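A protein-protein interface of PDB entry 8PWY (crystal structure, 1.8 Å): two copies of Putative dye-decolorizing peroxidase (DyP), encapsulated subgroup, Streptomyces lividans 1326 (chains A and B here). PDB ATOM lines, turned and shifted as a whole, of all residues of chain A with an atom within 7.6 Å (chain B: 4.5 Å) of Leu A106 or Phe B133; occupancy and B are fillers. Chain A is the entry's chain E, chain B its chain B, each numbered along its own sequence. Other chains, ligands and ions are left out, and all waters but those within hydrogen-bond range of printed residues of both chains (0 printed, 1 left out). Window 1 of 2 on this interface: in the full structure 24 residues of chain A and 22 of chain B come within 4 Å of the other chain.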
ATOM      1  N   SER A  13      25.400 -24.260   2.180  1.00  0.00           N
ATOM      2  CA  SER A  13      24.621 -23.887   1.024  1.00  0.00           C
ATOM      3  C   SER A  13      23.396 -23.051   1.421  1.00  0.00           C
ATOM      4  O   SER A  13      22.668 -22.594   0.543  1.00  0.00           O
ATOM      5  CB  SER A  13      24.257 -25.161   0.304  1.00  0.00           C
ATOM      6  OG  SER A  13      23.867 -26.083   1.290  1.00  0.00           O
ATOM      7  N   ALA A  14      23.162 -22.810   2.720  1.00  0.00           N
ATOM      8  CA  ALA A  14      22.040 -21.967   3.117  1.00  0.00           C
ATOM      9  C   ALA A  14      22.482 -21.015   4.211  1.00  0.00           C
ATOM     10  O   ALA A  14      23.367 -21.355   4.983  1.00  0.00           O
ATOM     11  CB  ALA A  14      20.895 -22.803   3.606  1.00  0.00           C
ATOM     12  N   ALA A  15      21.817 -19.863   4.283  1.00  0.00           N
ATOM     13  CA  ALA A  15      22.134 -18.872   5.298  1.00  0.00           C
ATOM     14  C   ALA A  15      20.916 -18.031   5.613  1.00  0.00           C
ATOM     15  O   ALA A  15      20.047 -17.839   4.784  1.00  0.00           O
ATOM     16  CB  ALA A  15      23.287 -17.993   4.878  1.00  0.00           C
ATOM     17  N   ILE A  16      20.863 -17.574   6.862  1.00  0.00           N
ATOM     18  CA  ILE A  16      19.995 -16.480   7.237  1.00  0.00           C
ATOM     19  C   ILE A  16      20.876 -15.369   7.794  1.00  0.00           C
ATOM     20  O   ILE A  16      21.719 -15.609   8.648  1.00  0.00           O
ATOM     21  CB  ILE A  16      18.917 -16.926   8.237  1.00  0.00           C
ATOM     22  CG1 ILE A  16      17.924 -17.884   7.580  1.00  0.00           C
ATOM     23  CG2 ILE A  16      18.232 -15.691   8.839  1.00  0.00           C
ATOM     24  CD1 ILE A  16      16.782 -18.310   8.431  1.00  0.00           C
ATOM     25  N   LEU A  54      25.474 -26.493  11.188  1.00  0.00           N
ATOM     26  CA  LEU A  54      24.853 -25.266  11.641  1.00  0.00           C
ATOM     27  C   LEU A  54      25.835 -24.454  12.467  1.00  0.00           C
ATOM     28  O   LEU A  54      26.460 -25.000  13.330  1.00  0.00           O
ATOM     29  CB  LEU A  54      23.624 -25.589  12.469  1.00  0.00           C
ATOM     30  CG  LEU A  54      22.968 -24.381  13.147  1.00  0.00           C
ATOM     31  CD1 LEU A  54      22.292 -23.476  12.123  1.00  0.00           C
ATOM     32  CD2 LEU A  54      21.977 -24.826  14.204  1.00  0.00           C
ATOM     33  N   ILE A 101      23.824 -16.814  10.241  1.00  0.00           N
ATOM     34  CA  ILE A 101      23.508 -18.203  10.531  1.00  0.00           C
ATOM     35  C   ILE A 101      23.677 -19.006   9.251  1.00  0.00           C
ATOM     36  O   ILE A 101      23.096 -18.636   8.241  1.00  0.00           O
ATOM     37  CB  ILE A 101      22.070 -18.297  11.067  1.00  0.00           C
ATOM     38  CG1 ILE A 101      21.872 -17.396  12.289  1.00  0.00           C
ATOM     39  CG2 ILE A 101      21.731 -19.738  11.353  1.00  0.00           C
ATOM     40  CD1 ILE A 101      20.447 -17.302  12.729  1.00  0.00           C
ATOM     41  N   ALA A 103      24.088 -23.106   7.446  1.00  0.00           N
ATOM     42  CA  ALA A 103      23.966 -24.538   7.567  1.00  0.00           C
ATOM     43  C   ALA A 103      23.885 -25.169   6.182  1.00  0.00           C
ATOM     44  O   ALA A 103      23.819 -24.485   5.163  1.00  0.00           O
ATOM     45  CB  ALA A 103      22.730 -24.854   8.367  1.00  0.00           C
ATOM     46  N   SER A 104      23.789 -26.504   6.155  1.00  0.00           N
ATOM     47  CA  SER A 104      23.582 -27.211   4.901  1.00  0.00           C
ATOM     48  C   SER A 104      22.127 -27.182   4.491  1.00  0.00           C
ATOM     49  O   SER A 104      21.836 -27.500   3.358  1.00  0.00           O
ATOM     50  CB  SER A 104      24.084 -28.606   4.968  1.00  0.00           C
ATOM     51  OG  SER A 104      23.326 -29.313   5.934  1.00  0.00           O
ATOM     52  N   ARG A 105      21.204 -26.745   5.348  1.00  0.00           N
ATOM     53  CA  ARG A 105      19.799 -26.675   4.959  1.00  0.00           C
ATOM     54  C   ARG A 105      19.132 -25.460   5.612  1.00  0.00           C
ATOM     55  O   ARG A 105      19.457 -25.133   6.746  1.00  0.00           O
ATOM     56  CB  ARG A 105      19.006 -27.850   5.541  1.00  0.00           C
ATOM     57  CG  ARG A 105      19.611 -29.241   5.531  1.00  0.00           C
ATOM     58  CD  ARG A 105      18.806 -30.258   6.353  1.00  0.00           C
ATOM     59  NE  ARG A 105      17.361 -30.208   6.089  1.00  0.00           N
ATOM     60  CZ  ARG A 105      16.585 -31.096   5.476  1.00  0.00           C
ATOM     61  NH1 ARG A 105      17.104 -32.113   4.822  1.00  0.00           N
ATOM     62  NH2 ARG A 105      15.287 -30.866   5.403  1.00  0.00           N
ATOM     63  N   LEU A 106      18.170 -24.838   4.934  1.00  0.00           N
ATOM     64  CA  LEU A 106      17.572 -23.617   5.411  1.00  0.00           C
ATOM     65  C   LEU A 106      16.795 -23.813   6.717  1.00  0.00           C
ATOM     66  O   LEU A 106      16.792 -22.924   7.577  1.00  0.00           O
ATOM     67  CB  LEU A 106      16.685 -23.058   4.320  1.00  0.00           C
ATOM     68  CG  LEU A 106      16.198 -21.634   4.603  1.00  0.00           C
ATOM     69  CD1 LEU A 106      17.385 -20.685   4.725  1.00  0.00           C
ATOM     70  CD2 LEU A 106      15.264 -21.119   3.520  1.00  0.00           C
ATOM     71  N   ASP A 107      16.155 -24.986   6.882  1.00  0.00           N
ATOM     72  CA  ASP A 107      15.319 -25.262   8.039  1.00  0.00           C
ATOM     73  C   ASP A 107      16.143 -25.155   9.310  1.00  0.00           C
ATOM     74  O   ASP A 107      15.620 -24.683  10.314  1.00  0.00           O
ATOM     75  CB  ASP A 107      14.610 -26.633   7.998  1.00  0.00           C
ATOM     76  CG  ASP A 107      15.558 -27.796   7.698  1.00  0.00           C
ATOM     77  OD1 ASP A 107      15.968 -27.811   6.444  1.00  0.00           O
ATOM     78  OD2 ASP A 107      15.962 -28.618   8.666  1.00  0.00           O
ATOM     79  N   LEU A 108      17.387 -25.612   9.312  1.00  0.00           N
ATOM     80  CA  LEU A 108      18.199 -25.490  10.511  1.00  0.00           C
ATOM     81  C   LEU A 108      18.503 -24.030  10.845  1.00  0.00           C
ATOM     82  O   LEU A 108      18.535 -23.660  12.033  1.00  0.00           O
ATOM     83  CB  LEU A 108      19.501 -26.247  10.320  1.00  0.00           C
ATOM     84  CG  LEU A 108      19.363 -27.765  10.410  1.00  0.00           C
ATOM     85  CD1 LEU A 108      20.721 -28.402  10.049  1.00  0.00           C
ATOM     86  CD2 LEU A 108      18.907 -28.177  11.821  1.00  0.00           C
ATOM     87  N   CYS A 109      18.784 -23.238   9.800  1.00  0.00           N
ATOM     88  CA  CYS A 109      19.003 -21.810   9.985  1.00  0.00           C
ATOM     89  C   CYS A 109      17.764 -21.189  10.611  1.00  0.00           C
ATOM     90  O   CYS A 109      17.866 -20.400  11.536  1.00  0.00           O
ATOM     91  CB  CYS A 109      19.324 -21.143   8.650  1.00  0.00           C
ATOM     92  SG  CYS A 109      20.865 -21.728   7.919  1.00  0.00           S
ATOM     93  N   PHE A 110      16.593 -21.554  10.078  1.00  0.00           N
ATOM     94  CA  PHE A 110      15.342 -20.976  10.511  1.00  0.00           C
ATOM     95  C   PHE A 110      15.047 -21.357  11.952  1.00  0.00           C
ATOM     96  O   PHE A 110      14.588 -20.535  12.739  1.00  0.00           O
ATOM     97  CB  PHE A 110      14.216 -21.363   9.544  1.00  0.00           C
ATOM     98  CG  PHE A 110      12.946 -20.584   9.724  1.00  0.00           C
ATOM     99  CD1 PHE A 110      12.777 -19.348   9.117  1.00  0.00           C
ATOM    100  CD2 PHE A 110      11.972 -20.999  10.611  1.00  0.00           C
ATOM    101  CE1 PHE A 110      11.675 -18.561   9.370  1.00  0.00           C
ATOM    102  CE2 PHE A 110      10.846 -20.239  10.826  1.00  0.00           C
ATOM    103  CZ  PHE A 110      10.683 -19.028  10.200  1.00  0.00           C
ATOM    104  N   ALA A 111      15.333 -22.588  12.321  1.00  0.00           N
ATOM    105  CA  ALA A 111      15.073 -23.051  13.679  1.00  0.00           C
ATOM    106  C   ALA A 111      15.900 -22.246  14.680  1.00  0.00           C
ATOM    107  O   ALA A 111      15.414 -21.835  15.729  1.00  0.00           O
ATOM    108  CB  ALA A 111      15.323 -24.549  13.778  1.00  0.00           C
ATOM    109  N   LEU A 112      17.177 -22.025  14.362  1.00  0.00           N
ATOM    110  CA  LEU A 112      18.041 -21.270  15.271  1.00  0.00           C
ATOM    111  C   LEU A 112      17.611 -19.790  15.310  1.00  0.00           C
ATOM    112  O   LEU A 112      17.569 -19.169  16.385  1.00  0.00           O
ATOM    113  CB  LEU A 112      19.510 -21.419  14.881  1.00  0.00           C
ATOM    114  CG  LEU A 112      20.488 -20.633  15.748  1.00  0.00           C
ATOM    115  CD1 LEU A 112      20.381 -21.011  17.219  1.00  0.00           C
ATOM    116  CD2 LEU A 112      21.914 -20.872  15.300  1.00  0.00           C
ATOM    117  N   ALA A 113      17.271 -19.219  14.144  1.00  0.00           N
ATOM    118  CA  ALA A 113      16.818 -17.841  14.107  1.00  0.00           C
ATOM    119  C   ALA A 113      15.545 -17.684  14.932  1.00  0.00           C
ATOM    120  O   ALA A 113      15.357 -16.672  15.588  1.00  0.00           O
ATOM    121  CB  ALA A 113      16.582 -17.400  12.686  1.00  0.00           C
ATOM    122  N   THR A 114      14.648 -18.684  14.884  1.00  0.00           N
ATOM    123  CA  THR A 114      13.429 -18.652  15.670  1.00  0.00           C
ATOM    124  C   THR A 114      13.729 -18.570  17.159  1.00  0.00           C
ATOM    125  O   THR A 114      13.111 -17.775  17.859  1.00  0.00           O
ATOM    126  CB  THR A 114      12.545 -19.861  15.370  1.00  0.00           C
ATOM    127  OG1 THR A 114      12.138 -19.688  14.022  1.00  0.00           O
ATOM    128  CG2 THR A 114      11.297 -19.911  16.213  1.00  0.00           C
ATOM    129  N   VAL A 130      17.391 -11.864   5.471  1.00  0.00           N
ATOM    130  CA  VAL A 130      17.615 -12.411   4.150  1.00  0.00           C
ATOM    131  C   VAL A 130      17.848 -13.924   4.295  1.00  0.00           C
ATOM    132  O   VAL A 130      18.628 -14.360   5.138  1.00  0.00           O
ATOM    133  CB  VAL A 130      18.826 -11.705   3.498  1.00  0.00           C
ATOM    134  CG1 VAL A 130      19.225 -12.364   2.195  1.00  0.00           C
ATOM    135  CG2 VAL A 130      18.543 -10.249   3.246  1.00  0.00           C
ATOM    136  N   HIS A 131      17.157 -14.686   3.464  1.00  0.00           N
ATOM    137  CA  HIS A 131      17.292 -16.129   3.366  1.00  0.00           C
ATOM    138  C   HIS A 131      18.089 -16.429   2.109  1.00  0.00           C
ATOM    139  O   HIS A 131      17.621 -16.174   1.024  1.00  0.00           O
ATOM    140  CB  HIS A 131      15.916 -16.829   3.353  1.00  0.00           C
ATOM    141  CG  HIS A 131      15.096 -16.609   4.582  1.00  0.00           C
ATOM    142  ND1 HIS A 131      13.850 -17.155   4.728  1.00  0.00           N
ATOM    143  CD2 HIS A 131      15.295 -15.859   5.690  1.00  0.00           C
ATOM    144  CE1 HIS A 131      13.296 -16.736   5.862  1.00  0.00           C
ATOM    145  NE2 HIS A 131      14.190 -15.979   6.489  1.00  0.00           N
ATOM    146  N   GLY A 132      19.319 -16.885   2.278  1.00  0.00           N
ATOM    147  CA  GLY A 132      20.253 -17.008   1.166  1.00  0.00           C
ATOM    148  C   GLY A 132      20.414 -18.469   0.774  1.00  0.00           C
ATOM    149  O   GLY A 132      20.263 -19.345   1.628  1.00  0.00           O
ATOM    150  N   PHE A 133      20.684 -18.712  -0.506  1.00  0.00           N
ATOM    151  CA  PHE A 133      20.847 -20.058  -1.031  1.00  0.00           C
ATOM    152  C   PHE A 133      21.950 -20.054  -2.085  1.00  0.00           C
ATOM    153  O   PHE A 133      21.979 -19.222  -2.958  1.00  0.00           O
ATOM    154  CB  PHE A 133      19.544 -20.556  -1.650  1.00  0.00           C
ATOM    155  CG  PHE A 133      18.830 -19.583  -2.573  1.00  0.00           C
ATOM    156  CD1 PHE A 133      19.168 -19.440  -3.915  1.00  0.00           C
ATOM    157  CD2 PHE A 133      17.805 -18.786  -2.077  1.00  0.00           C
ATOM    158  CE1 PHE A 133      18.519 -18.523  -4.732  1.00  0.00           C
ATOM    159  CE2 PHE A 133      17.121 -17.907  -2.913  1.00  0.00           C
ATOM    160  CZ  PHE A 133      17.485 -17.787  -4.244  1.00  0.00           C
ATOM    161  N   SER B  13      12.946 -31.585  -0.100  1.00  0.00           N
ATOM    162  CA  SER B  13      13.049 -30.799   1.111  1.00  0.00           C
ATOM    163  C   SER B  13      12.891 -29.310   0.808  1.00  0.00           C
ATOM    164  O   SER B  13      12.882 -28.532   1.752  1.00  0.00           O
ATOM    165  CB  SER B  13      14.366 -31.121   1.777  1.00  0.00           C
ATOM    166  OG  SER B  13      15.336 -31.156   0.749  1.00  0.00           O
ATOM    167  N   LEU B 106      16.761 -25.337  -2.657  1.00  0.00           N
ATOM    168  CA  LEU B 106      15.960 -24.182  -3.019  1.00  0.00           C
ATOM    169  C   LEU B 106      16.445 -23.476  -4.294  1.00  0.00           C
ATOM    170  O   LEU B 106      15.633 -22.997  -5.072  1.00  0.00           O
ATOM    171  CB  LEU B 106      15.965 -23.241  -1.820  1.00  0.00           C
ATOM    172  CG  LEU B 106      15.013 -22.071  -1.920  1.00  0.00           C
ATOM    173  CD1 LEU B 106      13.564 -22.553  -2.074  1.00  0.00           C
ATOM    174  CD2 LEU B 106      15.163 -21.201  -0.674  1.00  0.00           C
ATOM    175  N   HIS B 131       8.365 -19.784  -0.315  1.00  0.00           N
ATOM    176  CA  HIS B 131       9.586 -20.576  -0.368  1.00  0.00           C
ATOM    177  C   HIS B 131       9.522 -21.492   0.831  1.00  0.00           C
ATOM    178  O   HIS B 131       9.597 -21.017   1.944  1.00  0.00           O
ATOM    179  CB  HIS B 131      10.865 -19.713  -0.348  1.00  0.00           C
ATOM    180  CG  HIS B 131      10.971 -18.751  -1.490  1.00  0.00           C
ATOM    181  ND1 HIS B 131      12.115 -18.011  -1.711  1.00  0.00           N
ATOM    182  CD2 HIS B 131      10.114 -18.436  -2.513  1.00  0.00           C
ATOM    183  CE1 HIS B 131      11.923 -17.254  -2.792  1.00  0.00           C
ATOM    184  NE2 HIS B 131      10.719 -17.504  -3.295  1.00  0.00           N
ATOM    185  N   GLY B 132       9.301 -22.788   0.566  1.00  0.00           N
ATOM    186  CA  GLY B 132       9.080 -23.754   1.620  1.00  0.00           C
ATOM    187  C   GLY B 132      10.328 -24.559   1.901  1.00  0.00           C
ATOM    188  O   GLY B 132      11.141 -24.771   0.993  1.00  0.00           O
ATOM    189  N   PHE B 133      10.458 -25.010   3.149  1.00  0.00           N
ATOM    190  CA  PHE B 133      11.585 -25.832   3.573  1.00  0.00           C
ATOM    191  C   PHE B 133      11.098 -26.896   4.546  1.00  0.00           C
ATOM    192  O   PHE B 133      10.385 -26.587   5.454  1.00  0.00           O
ATOM    193  CB  PHE B 133      12.663 -24.974   4.225  1.00  0.00           C
ATOM    194  CG  PHE B 133      12.180 -23.957   5.235  1.00  0.00           C
ATOM    195  CD1 PHE B 133      11.990 -24.298   6.564  1.00  0.00           C
ATOM    196  CD2 PHE B 133      11.895 -22.657   4.854  1.00  0.00           C
ATOM    197  CE1 PHE B 133      11.540 -23.365   7.490  1.00  0.00           C
ATOM    198  CE2 PHE B 133      11.460 -21.723   5.767  1.00  0.00           C
ATOM    199  CZ  PHE B 133      11.276 -22.080   7.087  1.00  0.00           C
ATOM    200  N   LYS B 134      11.396 -28.174   4.344  1.00  0.00           N
ATOM    201  CA  LYS B 134      10.973 -29.183   5.295  1.00  0.00           C
ATOM    202  C   LYS B 134      12.044 -29.267   6.373  1.00  0.00           C
ATOM    203  O   LYS B 134      13.194 -29.096   6.091  1.00  0.00           O
ATOM    204  CB  LYS B 134      10.668 -30.537   4.634  1.00  0.00           C
ATOM    205  CG  LYS B 134       9.690 -31.412   5.429  1.00  0.00           C
ATOM    206  CD  LYS B 134       8.243 -30.812   5.585  1.00  0.00           C
ATOM    207  CE  LYS B 134       7.118 -31.695   6.105  1.00  0.00           C
ATOM    208  NZ  LYS B 134       7.033 -33.084   5.556  1.00  0.00           N
ATOM    209  N   TYR B 135      11.642 -29.479   7.620  1.00  0.00           N
ATOM    210  CA  TYR B 135      12.539 -29.776   8.721  1.00  0.00           C
ATOM    211  C   TYR B 135      13.129 -31.178   8.616  1.00  0.00           C
ATOM    212  O   TYR B 135      12.662 -32.036   7.878  1.00  0.00           O
ATOM    213  CB  TYR B 135      11.793 -29.689  10.030  1.00  0.00           C
ATOM    214  CG  TYR B 135      11.543 -28.247  10.447  1.00  0.00           C
ATOM    215  CD1 TYR B 135      12.519 -27.471  11.017  1.00  0.00           C
ATOM    216  CD2 TYR B 135      10.324 -27.670  10.234  1.00  0.00           C
ATOM    217  CE1 TYR B 135      12.288 -26.161  11.387  1.00  0.00           C
ATOM    218  CE2 TYR B 135      10.070 -26.363  10.584  1.00  0.00           C
ATOM    219  CZ  TYR B 135      11.059 -25.602  11.163  1.00  0.00           C
ATOM    220  OH  TYR B 135      10.742 -24.315  11.465  1.00  0.00           O
ATOM    221  N   MET B 240       4.349 -27.855   3.382  1.00  0.00           N
ATOM    222  CA  MET B 240       5.673 -27.281   3.568  1.00  0.00           C
ATOM    223  C   MET B 240       5.580 -26.149   4.580  1.00  0.00           C
ATOM    224  O   MET B 240       4.792 -25.223   4.439  1.00  0.00           O
ATOM    225  CB  MET B 240       6.226 -26.730   2.253  1.00  0.00           C
ATOM    226  CG  MET B 240       6.569 -27.800   1.238  1.00  0.00           C
ATOM    227  SD  MET B 240       7.809 -28.962   1.786  1.00  0.00           S
ATOM    228  CE  MET B 240       9.229 -27.966   1.476  1.00  0.00           C
ATOM    229  N   PRO B 241       6.471 -26.143   5.574  1.00  0.00           N
ATOM    230  CA  PRO B 241       6.703 -24.955   6.398  1.00  0.00           C
ATOM    231  C   PRO B 241       7.247 -23.793   5.608  1.00  0.00           C
ATOM    232  O   PRO B 241       7.951 -23.974   4.603  1.00  0.00           O
ATOM    233  CB  PRO B 241       7.798 -25.380   7.373  1.00  0.00           C
ATOM    234  CG  PRO B 241       7.695 -26.883   7.363  1.00  0.00           C
ATOM    235  CD  PRO B 241       7.298 -27.279   5.959  1.00  0.00           C
ATOM    236  N   PHE B 242       6.952 -22.599   6.094  1.00  0.00           N
ATOM    237  CA  PHE B 242       7.547 -21.400   5.529  1.00  0.00           C
ATOM    238  C   PHE B 242       7.478 -20.351   6.610  1.00  0.00           C
ATOM    239  O   PHE B 242       6.710 -20.497   7.572  1.00  0.00           O
ATOM    240  CB  PHE B 242       6.811 -20.910   4.288  1.00  0.00           C
ATOM    241  CG  PHE B 242       5.431 -20.371   4.547  1.00  0.00           C
ATOM    242  CD1 PHE B 242       4.330 -21.215   4.616  1.00  0.00           C
ATOM    243  CD2 PHE B 242       5.226 -19.018   4.775  1.00  0.00           C
ATOM    244  CE1 PHE B 242       3.074 -20.719   4.906  1.00  0.00           C
ATOM    245  CE2 PHE B 242       3.966 -18.517   5.067  1.00  0.00           C
ATOM    246  CZ  PHE B 242       2.901 -19.374   5.136  1.00  0.00           C
ATOM    247  N   GLY B 243       8.270 -19.288   6.440  1.00  0.00           N
ATOM    248  CA  GLY B 243       8.054 -18.160   7.312  1.00  0.00           C
ATOM    249  C   GLY B 243       9.123 -17.100   7.256  1.00  0.00           C
ATOM    250  O   GLY B 243      10.060 -17.141   6.465  1.00  0.00           O
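Of the printed residues of chain B, Leu A106 touches Phe B133.
Phe B133 touches just these residues of chain A: Leu A106, Asp A107 and Phe A110.
Of the printed residues of chain A, Ser B13 touches Arg A105.
Of the printed residues of chain A, Leu B106 touches Phe A133.
Of the printed residues of chain B, Phe A110 touches Phe B133 (3.5 Å), Tyr B135 (3.6 Å) and Gly B243 (3.6 Å).
Ile A16 touches none of the printed residues of chain B.
The nearest residue of chain B that does not touch Leu A106 is Leu B106 (4.2 Å).
NH2 of Arg A105 is in hydrogen-bond range of O of Lys B134, 2.8 Å away.
The side-chain carboxylate (OD1) of Asp A107 sits close to the backbone carbonyl oxygen (O) of Lys B134 (3.1 Å).
Among the printed residues, merely in contact across the chains: His A131 with Gly B243 (3.3 Å), Phe A110 with Phe B133 (3.5 Å), Asp A107 with Tyr B135 (3.6 Å), Phe A110 with Gly B243 (3.6 Å), Phe A110 with Tyr B135 (3.6 Å), Arg A105 with Ser B13 (3.7 Å), Asp A107 with Phe B133 (3.8 Å), Arg A105 with Tyr B135 (3.8 Å), Phe A133 with Leu B106 (3.8 Å) and Leu A106 with Phe B133 (3.9 Å).
The backbone NH (N) of Lys B134 lies within hydrogen-bond range of the backbone carbonyl oxygen (O) of Ser B13 (3.0 Å).
The backbone carbonyl oxygen (O) of Pro B241 lies within hydrogen-bond range of the backbone NH (N) of Phe B133.
The guanidinium group of Arg A105 is in salt-bridge range of the side-chain carboxylate of Asp A107 (2.8 Å).
The side-chain hydroxyl of Thr A114 is in hydrogen-bond range of the backbone carbonyl oxygen of Phe A110, at 2.9 Å.
Of the 11 printed residues of chain B, 6 touch a printed residue of chain A.
Hydrophobic or aromatic side chains of chain B that line the printed part of chain A: Leu B106, Phe B133 and Tyr B135.
Hydrophobic or aromatic side chains of chain A that line the printed part of chain B: Leu A106, Phe A110, His A131 and Phe A133.
Among the printed residues, 12 pairs touch across the chains.
Among the printed residues, no Asp or Glu carboxylate lies within 4 Å of a Lys or Arg side-chain nitrogen of the other chain.
Leu A106 touches Phe B133, and with the chains exchanged Phe A133 touches Leu B106.
Of the 12 pairs that touch across the chains among the printed residues, 2 have their exchanged pair printed and touching as well.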
